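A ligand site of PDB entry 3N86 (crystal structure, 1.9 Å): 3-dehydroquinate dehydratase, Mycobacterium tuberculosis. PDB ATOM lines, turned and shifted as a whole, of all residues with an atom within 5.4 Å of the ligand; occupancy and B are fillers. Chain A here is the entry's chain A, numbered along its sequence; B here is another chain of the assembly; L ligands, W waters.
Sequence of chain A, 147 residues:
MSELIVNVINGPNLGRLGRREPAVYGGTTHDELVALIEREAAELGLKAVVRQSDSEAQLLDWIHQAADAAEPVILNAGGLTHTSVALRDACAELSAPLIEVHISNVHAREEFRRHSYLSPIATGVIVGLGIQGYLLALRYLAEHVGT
OD2 of Asp 89 of chain B sits close to O5 of the ligand, at 2.6 Å. The backbone NH (N) of Ser 104 lies within hydrogen-bond range of an oxygen (O3) of the ligand (2.7 Å). O3 of the ligand lies within hydrogen-bond range of OG of Ser 104, at 2.6 Å. A ring nitrogen (ND1) of His 102 sits at hydrogen-bond distance from an oxygen (O6) of the ligand (2.7 Å). A ring nitrogen (NE2) of His 82 sits at hydrogen-bond distance from an oxygen (O4) of the ligand, at 2.7 Å. O4 of the ligand is in hydrogen-bond range of NH1 of Arg 113 (2.8 Å). The side-chain amide nitrogen (ND2) of Asn 76 sits at hydrogen-bond distance from an oxygen (O2) of the ligand, 2.8 Å away. The backbone NH (N) of Ile 103 is in hydrogen-bond range of an oxygen (O2) of the ligand (2.9 Å). O1 of the ligand lies within hydrogen-bond range of ND2 of Asn 13 (3.1 Å). An oxygen (O5) of the ligand lies within hydrogen-bond range of the backbone NH (N) of Gly 79 (3.1 Å).
The side-chain carboxylate (OD1) of Asp 89 of chain B is in salt-bridge range of the guanidinium group (NH2) of Arg 113 (2.7 Å). OG of Ser 104 lies within hydrogen-bond range of NH1 of Arg 109 (2.9 Å). N of Gly 78 lies within hydrogen-bond range of OD1 of Asn 76 (3.1 Å). ND2 of Asn 13 is in hydrogen-bond range of O of Ala 86 of chain B (2.9 Å). NH1 of Arg 109 is in hydrogen-bond range of OH of Tyr 25 (2.9 Å). OE1 of Glu 93 of chain B is in salt-bridge range of NH1 of Arg 20. The guanidinium group (NH2) of Arg 16 is in salt-bridge range of the side-chain carboxylate (OE1) of Glu 93 of chain B. OG1 of Thr 81 sits at hydrogen-bond distance from O of Gly 78 (2.7 Å).
O of Pro 12 touches O1 of the ligand, 3.9 Å away. Leu 14 touches the ligand. Arg 16 touches the ligand (CB to C6, 3.7 Å). O of Arg 20 touches C6 of the ligand, 3.7 Å away. CG of Glu 21 touches C4 of the ligand, 3.6 Å away. OH of Tyr 25 touches C12 of the ligand (3.3 Å). Gly 78 touches the ligand (C to O5, 3.4 Å). CG1 of Val 106 touches C9 of the ligand, 3.6 Å away. Val 85 of chain B touches the ligand (CG1 to O5, 3.9 Å). OE2 of Glu 93 of chain B touches C4 of the ligand, 3.3 Å away. Hydrophobic or aromatic side chains that line the ligand: Leu 14, Tyr 25, His 82, His 102, Ile 103, Val 106 and Val 85 of chain B. Within 4 Å of the ligand: Pro 12, Asn 13, Leu 14, Arg 16, Arg 20, Glu 21, Tyr 25, Asn 76, Gly 78, Gly 79, His 82, His 102, Ile 103, Ser 104, Val 106, Arg 113, Val 85 of chain B, Asp 89 of chain B and Glu 93 of chain B.
Water W1 lies within hydrogen-bond range of N of Gly 79 (2.8 Å), O of Pro 12 (2.9 Å), O1 of the ligand (3.2 Å) and ND2 of Asn 13 (3.3 Å).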
ATOM      1  N   PRO A  12     -15.137 -29.110 -12.129  1.00  0.00           N
ATOM      2  CA  PRO A  12     -14.684 -28.253 -13.226  1.00  0.00           C
ATOM      3  C   PRO A  12     -13.234 -28.472 -13.648  1.00  0.00           C
ATOM      4  O   PRO A  12     -12.363 -28.673 -12.805  1.00  0.00           O
ATOM      5  CB  PRO A  12     -14.839 -26.852 -12.678  1.00  0.00           C
ATOM      6  CG  PRO A  12     -15.752 -26.966 -11.515  1.00  0.00           C
ATOM      7  CD  PRO A  12     -15.820 -28.360 -11.051  1.00  0.00           C
ATOM      8  N   ASN A  13     -13.039 -28.469 -14.993  1.00  0.00           N
ATOM      9  CA  ASN A  13     -11.745 -28.582 -15.625  1.00  0.00           C
ATOM     10  C   ASN A  13     -11.240 -30.006 -15.762  1.00  0.00           C
ATOM     11  O   ASN A  13     -10.285 -30.261 -16.528  1.00  0.00           O
ATOM     12  CB  ASN A  13     -10.684 -27.717 -14.954  1.00  0.00           C
ATOM     13  CG  ASN A  13     -11.120 -26.253 -14.822  1.00  0.00           C
ATOM     14  OD1 ASN A  13     -11.776 -25.700 -15.719  1.00  0.00           O
ATOM     15  ND2 ASN A  13     -10.746 -25.600 -13.711  1.00  0.00           N
ATOM     16  N   LEU A  14     -11.826 -30.912 -14.996  1.00  0.00           N
ATOM     17  CA  LEU A  14     -11.228 -32.255 -14.898  1.00  0.00           C
ATOM     18  C   LEU A  14     -11.490 -33.060 -16.168  1.00  0.00           C
ATOM     19  O   LEU A  14     -10.890 -34.128 -16.333  1.00  0.00           O
ATOM     20  CB  LEU A  14     -11.686 -33.023 -13.647  1.00  0.00           C
ATOM     21  CG  LEU A  14     -11.098 -32.359 -12.378  1.00  0.00           C
ATOM     22  CD1 LEU A  14     -11.858 -32.845 -11.189  1.00  0.00           C
ATOM     23  CD2 LEU A  14      -9.652 -32.686 -12.210  1.00  0.00           C
ATOM     24  N   ARG A  16     -10.298 -32.199 -18.689  1.00  0.00           N
ATOM     25  CA  ARG A  16      -9.009 -32.010 -19.372  1.00  0.00           C
ATOM     26  C   ARG A  16      -7.812 -32.766 -18.821  1.00  0.00           C
ATOM     27  O   ARG A  16      -6.637 -32.544 -19.237  1.00  0.00           O
ATOM     28  CB  ARG A  16      -8.679 -30.531 -19.398  1.00  0.00           C
ATOM     29  CG  ARG A  16      -9.763 -29.807 -20.215  1.00  0.00           C
ATOM     30  CD  ARG A  16      -9.617 -28.275 -20.031  1.00  0.00           C
ATOM     31  NE  ARG A  16      -8.417 -27.744 -20.671  1.00  0.00           N
ATOM     32  CZ  ARG A  16      -8.197 -27.644 -21.992  1.00  0.00           C
ATOM     33  NH1 ARG A  16      -9.073 -28.095 -22.890  1.00  0.00           N
ATOM     34  NH2 ARG A  16      -7.054 -27.134 -22.405  1.00  0.00           N
ATOM     35  N   LEU A  17      -8.099 -33.684 -17.904  1.00  0.00           N
ATOM     36  CA  LEU A  17      -7.076 -34.479 -17.282  1.00  0.00           C
ATOM     37  C   LEU A  17      -6.178 -35.095 -18.345  1.00  0.00           C
ATOM     38  O   LEU A  17      -6.660 -35.586 -19.412  1.00  0.00           O
ATOM     39  CB  LEU A  17      -7.694 -35.612 -16.464  1.00  0.00           C
ATOM     40  CG  LEU A  17      -8.029 -35.273 -15.015  1.00  0.00           C
ATOM     41  CD1 LEU A  17      -8.734 -36.495 -14.450  1.00  0.00           C
ATOM     42  CD2 LEU A  17      -6.754 -34.929 -14.199  1.00  0.00           C
ATOM     43  N   ARG A  20      -3.774 -32.241 -20.440  1.00  0.00           N
ATOM     44  CA  ARG A  20      -3.420 -30.876 -20.024  1.00  0.00           C
ATOM     45  C   ARG A  20      -2.962 -30.912 -18.537  1.00  0.00           C
ATOM     46  O   ARG A  20      -3.419 -31.785 -17.775  1.00  0.00           O
ATOM     47  CB  ARG A  20      -4.675 -30.013 -20.208  1.00  0.00           C
ATOM     48  CG  ARG A  20      -5.224 -30.023 -21.672  1.00  0.00           C
ATOM     49  CD  ARG A  20      -4.208 -29.404 -22.684  1.00  0.00           C
ATOM     50  NE  ARG A  20      -3.732 -28.090 -22.171  1.00  0.00           N
ATOM     51  CZ  ARG A  20      -2.920 -27.218 -22.791  1.00  0.00           C
ATOM     52  NH1 ARG A  20      -2.605 -26.082 -22.189  1.00  0.00           N
ATOM     53  NH2 ARG A  20      -2.417 -27.471 -24.004  1.00  0.00           N
ATOM     54  N   GLU A  21      -2.055 -30.024 -18.132  1.00  0.00           N
ATOM     55  CA  GLU A  21      -1.561 -30.010 -16.722  1.00  0.00           C
ATOM     56  C   GLU A  21      -1.028 -31.390 -16.198  1.00  0.00           C
ATOM     57  O   GLU A  21      -1.188 -31.691 -15.022  1.00  0.00           O
ATOM     58  CB  GLU A  21      -2.611 -29.401 -15.764  1.00  0.00           C
ATOM     59  CG  GLU A  21      -3.031 -27.965 -16.091  1.00  0.00           C
ATOM     60  CD  GLU A  21      -1.946 -26.930 -15.711  1.00  0.00           C
ATOM     61  OE1 GLU A  21      -0.987 -26.785 -16.463  1.00  0.00           O
ATOM     62  OE2 GLU A  21      -2.082 -26.261 -14.642  1.00  0.00           O
ATOM     63  N   TYR A  25      -1.666 -33.064 -12.352  1.00  0.00           N
ATOM     64  CA  TYR A  25      -2.831 -33.958 -12.182  1.00  0.00           C
ATOM     65  C   TYR A  25      -2.675 -35.316 -12.840  1.00  0.00           C
ATOM     66  O   TYR A  25      -3.621 -36.104 -12.868  1.00  0.00           O
ATOM     67  CB  TYR A  25      -4.131 -33.249 -12.679  1.00  0.00           C
ATOM     68  CG  TYR A  25      -4.468 -31.999 -11.832  1.00  0.00           C
ATOM     69  CD1 TYR A  25      -4.385 -30.718 -12.392  1.00  0.00           C
ATOM     70  CD2 TYR A  25      -4.808 -32.109 -10.445  1.00  0.00           C
ATOM     71  CE1 TYR A  25      -4.667 -29.518 -11.596  1.00  0.00           C
ATOM     72  CE2 TYR A  25      -5.089 -30.926  -9.653  1.00  0.00           C
ATOM     73  CZ  TYR A  25      -4.989 -29.667 -10.243  1.00  0.00           C
ATOM     74  OH  TYR A  25      -5.230 -28.534  -9.531  1.00  0.00           O
ATOM     75  N   ASN A  76     -14.701 -35.639  -6.778  1.00  0.00           N
ATOM     76  CA  ASN A  76     -13.532 -34.732  -6.849  1.00  0.00           C
ATOM     77  C   ASN A  76     -14.114 -33.417  -7.385  1.00  0.00           C
ATOM     78  O   ASN A  76     -14.396 -33.274  -8.574  1.00  0.00           O
ATOM     79  CB  ASN A  76     -12.389 -35.280  -7.769  1.00  0.00           C
ATOM     80  CG  ASN A  76     -11.228 -34.315  -7.833  1.00  0.00           C
ATOM     81  OD1 ASN A  76     -11.384 -33.165  -7.406  1.00  0.00           O
ATOM     82  ND2 ASN A  76     -10.121 -34.706  -8.467  1.00  0.00           N
ATOM     83  N   ALA A  77     -14.352 -32.472  -6.478  1.00  0.00           N
ATOM     84  CA  ALA A  77     -15.072 -31.269  -6.842  1.00  0.00           C
ATOM     85  C   ALA A  77     -14.171 -30.208  -7.489  1.00  0.00           C
ATOM     86  O   ALA A  77     -14.687 -29.158  -7.890  1.00  0.00           O
ATOM     87  CB  ALA A  77     -15.822 -30.703  -5.605  1.00  0.00           C
ATOM     88  N   GLY A  78     -12.858 -30.460  -7.647  1.00  0.00           N
ATOM     89  CA  GLY A  78     -12.010 -29.460  -8.297  1.00  0.00           C
ATOM     90  C   GLY A  78     -11.968 -28.225  -7.419  1.00  0.00           C
ATOM     91  O   GLY A  78     -12.027 -28.364  -6.176  1.00  0.00           O
ATOM     92  N   GLY A  79     -11.943 -27.049  -8.056  1.00  0.00           N
ATOM     93  CA  GLY A  79     -11.815 -25.765  -7.318  1.00  0.00           C
ATOM     94  C   GLY A  79     -13.005 -25.581  -6.351  1.00  0.00           C
ATOM     95  O   GLY A  79     -12.856 -24.864  -5.366  1.00  0.00           O
ATOM     96  N   THR A  81     -14.266 -27.527  -4.314  1.00  0.00           N
ATOM     97  CA  THR A  81     -13.942 -28.030  -2.970  1.00  0.00           C
ATOM     98  C   THR A  81     -13.802 -26.956  -1.912  1.00  0.00           C
ATOM     99  O   THR A  81     -14.201 -27.141  -0.728  1.00  0.00           O
ATOM    100  CB  THR A  81     -12.564 -28.765  -3.027  1.00  0.00           C
ATOM    101  OG1 THR A  81     -12.704 -29.805  -3.997  1.00  0.00           O
ATOM    102  CG2 THR A  81     -12.227 -29.409  -1.710  1.00  0.00           C
ATOM    103  N   HIS A  82     -13.105 -25.879  -2.293  1.00  0.00           N
ATOM    104  CA  HIS A  82     -12.675 -24.859  -1.342  1.00  0.00           C
ATOM    105  C   HIS A  82     -13.620 -23.660  -1.314  1.00  0.00           C
ATOM    106  O   HIS A  82     -13.410 -22.709  -0.555  1.00  0.00           O
ATOM    107  CB  HIS A  82     -11.280 -24.371  -1.728  1.00  0.00           C
ATOM    108  CG  HIS A  82     -10.367 -25.493  -2.175  1.00  0.00           C
ATOM    109  ND1 HIS A  82      -9.802 -26.389  -1.300  1.00  0.00           N
ATOM    110  CD2 HIS A  82      -9.848 -25.797  -3.395  1.00  0.00           C
ATOM    111  CE1 HIS A  82      -9.015 -27.223  -1.968  1.00  0.00           C
ATOM    112  NE2 HIS A  82      -9.039 -26.892  -3.240  1.00  0.00           N
ATOM    113  N   VAL A 101     -12.148 -37.007  -3.048  1.00  0.00           N
ATOM    114  CA  VAL A 101     -10.878 -37.433  -3.590  1.00  0.00           C
ATOM    115  C   VAL A 101     -10.190 -36.208  -4.173  1.00  0.00           C
ATOM    116  O   VAL A 101     -10.845 -35.421  -4.907  1.00  0.00           O
ATOM    117  CB  VAL A 101     -11.088 -38.533  -4.729  1.00  0.00           C
ATOM    118  CG1 VAL A 101      -9.865 -38.707  -5.575  1.00  0.00           C
ATOM    119  CG2 VAL A 101     -11.509 -39.923  -4.111  1.00  0.00           C
ATOM    120  N   HIS A 102      -8.887 -36.049  -3.883  1.00  0.00           N
ATOM    121  CA  HIS A 102      -8.045 -35.152  -4.651  1.00  0.00           C
ATOM    122  C   HIS A 102      -6.854 -35.908  -5.250  1.00  0.00           C
ATOM    123  O   HIS A 102      -6.182 -36.578  -4.560  1.00  0.00           O
ATOM    124  CB  HIS A 102      -7.582 -34.002  -3.744  1.00  0.00           C
ATOM    125  CG  HIS A 102      -8.747 -33.231  -3.176  1.00  0.00           C
ATOM    126  ND1 HIS A 102      -9.506 -32.381  -3.949  1.00  0.00           N
ATOM    127  CD2 HIS A 102      -9.361 -33.298  -1.968  1.00  0.00           C
ATOM    128  CE1 HIS A 102     -10.507 -31.899  -3.228  1.00  0.00           C
ATOM    129  NE2 HIS A 102     -10.450 -32.443  -2.024  1.00  0.00           N
ATOM    130  N   ILE A 103      -6.605 -35.718  -6.543  1.00  0.00           N
ATOM    131  CA  ILE A 103      -5.503 -36.338  -7.264  1.00  0.00           C
ATOM    132  C   ILE A 103      -4.191 -35.747  -6.710  1.00  0.00           C
ATOM    133  O   ILE A 103      -3.256 -36.505  -6.417  1.00  0.00           O
ATOM    134  CB  ILE A 103      -5.638 -36.051  -8.760  1.00  0.00           C
ATOM    135  CG1 ILE A 103      -6.922 -36.677  -9.334  1.00  0.00           C
ATOM    136  CG2 ILE A 103      -4.328 -36.437  -9.567  1.00  0.00           C
ATOM    137  CD1 ILE A 103      -7.303 -36.138 -10.747  1.00  0.00           C
ATOM    138  N   SER A 104      -4.109 -34.403  -6.547  1.00  0.00           N
ATOM    139  CA  SER A 104      -2.873 -33.767  -6.050  1.00  0.00           C
ATOM    140  C   SER A 104      -2.868 -33.695  -4.522  1.00  0.00           C
ATOM    141  O   SER A 104      -3.921 -33.870  -3.869  1.00  0.00           O
ATOM    142  CB  SER A 104      -2.713 -32.330  -6.627  1.00  0.00           C
ATOM    143  OG  SER A 104      -3.623 -31.411  -6.048  1.00  0.00           O
ATOM    144  N   ASN A 105      -1.673 -33.463  -3.958  1.00  0.00           N
ATOM    145  CA  ASN A 105      -1.594 -33.247  -2.523  1.00  0.00           C
ATOM    146  C   ASN A 105      -1.878 -31.789  -2.246  1.00  0.00           C
ATOM    147  O   ASN A 105      -1.004 -30.904  -2.374  1.00  0.00           O
ATOM    148  CB  ASN A 105      -0.258 -33.701  -1.963  1.00  0.00           C
ATOM    149  CG  ASN A 105      -0.203 -33.548  -0.464  1.00  0.00           C
ATOM    150  OD1 ASN A 105      -1.136 -33.008   0.154  1.00  0.00           O
ATOM    151  ND2 ASN A 105       0.879 -34.055   0.136  1.00  0.00           N
ATOM    152  N   VAL A 106      -3.133 -31.541  -1.931  1.00  0.00           N
ATOM    153  CA  VAL A 106      -3.583 -30.197  -1.617  1.00  0.00           C
ATOM    154  C   VAL A 106      -2.836 -29.538  -0.440  1.00  0.00           C
ATOM    155  O   VAL A 106      -2.910 -28.320  -0.310  1.00  0.00           O
ATOM    156  CB  VAL A 106      -5.149 -30.122  -1.366  1.00  0.00           C
ATOM    157  CG1 VAL A 106      -5.940 -30.451  -2.719  1.00  0.00           C
ATOM    158  CG2 VAL A 106      -5.609 -31.064  -0.235  1.00  0.00           C
ATOM    159  N   ARG A 109       0.526 -27.473  -1.596  1.00  0.00           N
ATOM    160  CA  ARG A 109       0.296 -26.419  -2.586  1.00  0.00           C
ATOM    161  C   ARG A 109       0.023 -25.045  -1.872  1.00  0.00           C
ATOM    162  O   ARG A 109       0.602 -24.765  -0.819  1.00  0.00           O
ATOM    163  CB  ARG A 109      -0.821 -26.862  -3.522  1.00  0.00           C
ATOM    164  CG  ARG A 109      -0.428 -28.195  -4.259  1.00  0.00           C
ATOM    165  CD  ARG A 109      -1.419 -28.651  -5.341  1.00  0.00           C
ATOM    166  NE  ARG A 109      -1.674 -27.599  -6.348  1.00  0.00           N
ATOM    167  CZ  ARG A 109      -2.665 -27.693  -7.255  1.00  0.00           C
ATOM    168  NH1 ARG A 109      -3.490 -28.781  -7.241  1.00  0.00           N
ATOM    169  NH2 ARG A 109      -2.846 -26.727  -8.156  1.00  0.00           N
ATOM    170  N   ARG A 113      -5.791 -24.095  -0.506  1.00  0.00           N
ATOM    171  CA  ARG A 113      -6.202 -25.500  -0.868  1.00  0.00           C
ATOM    172  C   ARG A 113      -6.238 -26.402   0.320  1.00  0.00           C
ATOM    173  O   ARG A 113      -6.671 -27.542   0.191  1.00  0.00           O
ATOM    174  CB  ARG A 113      -5.357 -26.163  -1.974  1.00  0.00           C
ATOM    175  CG  ARG A 113      -5.194 -25.275  -3.228  1.00  0.00           C
ATOM    176  CD  ARG A 113      -4.565 -26.086  -4.412  1.00  0.00           C
ATOM    177  NE  ARG A 113      -4.290 -25.109  -5.484  1.00  0.00           N
ATOM    178  CZ  ARG A 113      -5.189 -24.830  -6.437  1.00  0.00           C
ATOM    179  NH1 ARG A 113      -6.363 -25.499  -6.467  1.00  0.00           N
ATOM    180  NH2 ARG A 113      -4.904 -23.908  -7.367  1.00  0.00           N
ATOM    181  N   VAL B  85     -11.985 -20.528  -7.466  1.00  0.00           N
ATOM    182  CA  VAL B  85     -10.688 -21.246  -7.614  1.00  0.00           C
ATOM    183  C   VAL B  85     -10.740 -22.054  -8.926  1.00  0.00           C
ATOM    184  O   VAL B  85      -9.718 -22.249  -9.603  1.00  0.00           O
ATOM    185  CB  VAL B  85     -10.462 -22.245  -6.434  1.00  0.00           C
ATOM    186  CG1 VAL B  85      -9.248 -23.272  -6.729  1.00  0.00           C
ATOM    187  CG2 VAL B  85     -10.215 -21.403  -5.093  1.00  0.00           C
ATOM    188  N   ALA B  86     -11.931 -22.552  -9.262  1.00  0.00           N
ATOM    189  CA  ALA B  86     -12.111 -23.254 -10.547  1.00  0.00           C
ATOM    190  C   ALA B  86     -11.665 -22.406 -11.711  1.00  0.00           C
ATOM    191  O   ALA B  86     -10.972 -22.914 -12.628  1.00  0.00           O
ATOM    192  CB  ALA B  86     -13.554 -23.712 -10.713  1.00  0.00           C
ATOM    193  N   ASP B  89      -7.864 -22.080 -11.644  1.00  0.00           N
ATOM    194  CA  ASP B  89      -7.226 -23.311 -12.171  1.00  0.00           C
ATOM    195  C   ASP B  89      -7.299 -23.410 -13.699  1.00  0.00           C
ATOM    196  O   ASP B  89      -6.350 -23.892 -14.336  1.00  0.00           O
ATOM    197  CB  ASP B  89      -7.766 -24.522 -11.408  1.00  0.00           C
ATOM    198  CG  ASP B  89      -7.174 -24.564  -9.964  1.00  0.00           C
ATOM    199  OD1 ASP B  89      -6.109 -23.932  -9.773  1.00  0.00           O
ATOM    200  OD2 ASP B  89      -7.662 -25.178  -9.050  1.00  0.00           O
ATOM    201  N   ALA B  90      -8.416 -22.955 -14.288  1.00  0.00           N
ATOM    202  CA  ALA B  90      -8.536 -23.028 -15.764  1.00  0.00           C
ATOM    203  C   ALA B  90      -7.560 -22.041 -16.354  1.00  0.00           C
ATOM    204  O   ALA B  90      -6.871 -22.357 -17.330  1.00  0.00           O
ATOM    205  CB  ALA B  90      -9.927 -22.726 -16.221  1.00  0.00           C
ATOM    206  N   GLU B  93      -3.640 -22.819 -16.666  1.00  0.00           N
ATOM    207  CA  GLU B  93      -3.237 -23.715 -17.743  1.00  0.00           C
ATOM    208  C   GLU B  93      -2.860 -22.880 -18.970  1.00  0.00           C
ATOM    209  O   GLU B  93      -2.179 -23.372 -19.829  1.00  0.00           O
ATOM    210  CB  GLU B  93      -4.450 -24.611 -18.111  1.00  0.00           C
ATOM    211  CG  GLU B  93      -4.136 -25.727 -19.056  1.00  0.00           C
ATOM    212  CD  GLU B  93      -5.324 -26.313 -19.729  1.00  0.00           C
ATOM    213  OE1 GLU B  93      -5.079 -26.879 -20.783  1.00  0.00           O
ATOM    214  OE2 GLU B  93      -6.495 -26.226 -19.260  1.00  0.00           O
HETATM  215  O1  LIG L   1      -8.694 -27.478 -12.422  1.00  0.00           O
HETATM  216  O2  LIG L   1      -7.769 -33.310  -7.679  1.00  0.00           O
HETATM  217  O3  LIG L   1      -5.965 -32.470  -6.623  1.00  0.00           O
HETATM  218  O4  LIG L   1      -7.382 -27.797  -5.155  1.00  0.00           O
HETATM  219  O5  LIG L   1      -8.825 -27.067  -7.640  1.00  0.00           O
HETATM  220  O6  LIG L   1      -9.250 -31.441  -6.420  1.00  0.00           O
HETATM  221  C1  LIG L   1      -8.616 -29.389 -11.053  1.00  0.00           C
HETATM  222  C2  LIG L   1      -8.514 -28.471  -9.874  1.00  0.00           C
HETATM  223  C3  LIG L   1      -8.152 -30.471  -8.360  1.00  0.00           C
HETATM  224  C4  LIG L   1      -6.421 -28.583 -17.000  1.00  0.00           C
HETATM  225  C5  LIG L   1      -6.907 -27.529 -16.211  1.00  0.00           C
HETATM  226  C6  LIG L   1      -6.372 -29.914 -16.523  1.00  0.00           C
HETATM  227  C7  LIG L   1      -7.332 -27.836 -14.917  1.00  0.00           C
HETATM  228  C8  LIG L   1      -6.818 -30.228 -15.233  1.00  0.00           C
HETATM  229  C9  LIG L   1      -7.200 -30.114  -6.022  1.00  0.00           C
HETATM  230  N1  LIG L   1      -7.735 -29.476 -13.199  1.00  0.00           N
HETATM  231  C10 LIG L   1      -8.309 -28.642 -12.301  1.00  0.00           C
HETATM  232  C11 LIG L   1      -7.130 -32.377  -7.121  1.00  0.00           C
HETATM  233  C12 LIG L   1      -8.266 -29.117  -8.517  1.00  0.00           C
HETATM  234  C13 LIG L   1      -7.299 -29.165 -14.457  1.00  0.00           C
HETATM  235  C14 LIG L   1      -7.957 -28.765  -6.029  1.00  0.00           C
HETATM  236  C15 LIG L   1      -8.261 -28.273  -7.452  1.00  0.00           C
HETATM  237  C16 LIG L   1      -7.907 -31.097  -6.991  1.00  0.00           C
HETATM  238  O   HOH W   1     -11.308 -26.913 -10.730  1.00  0.00           O
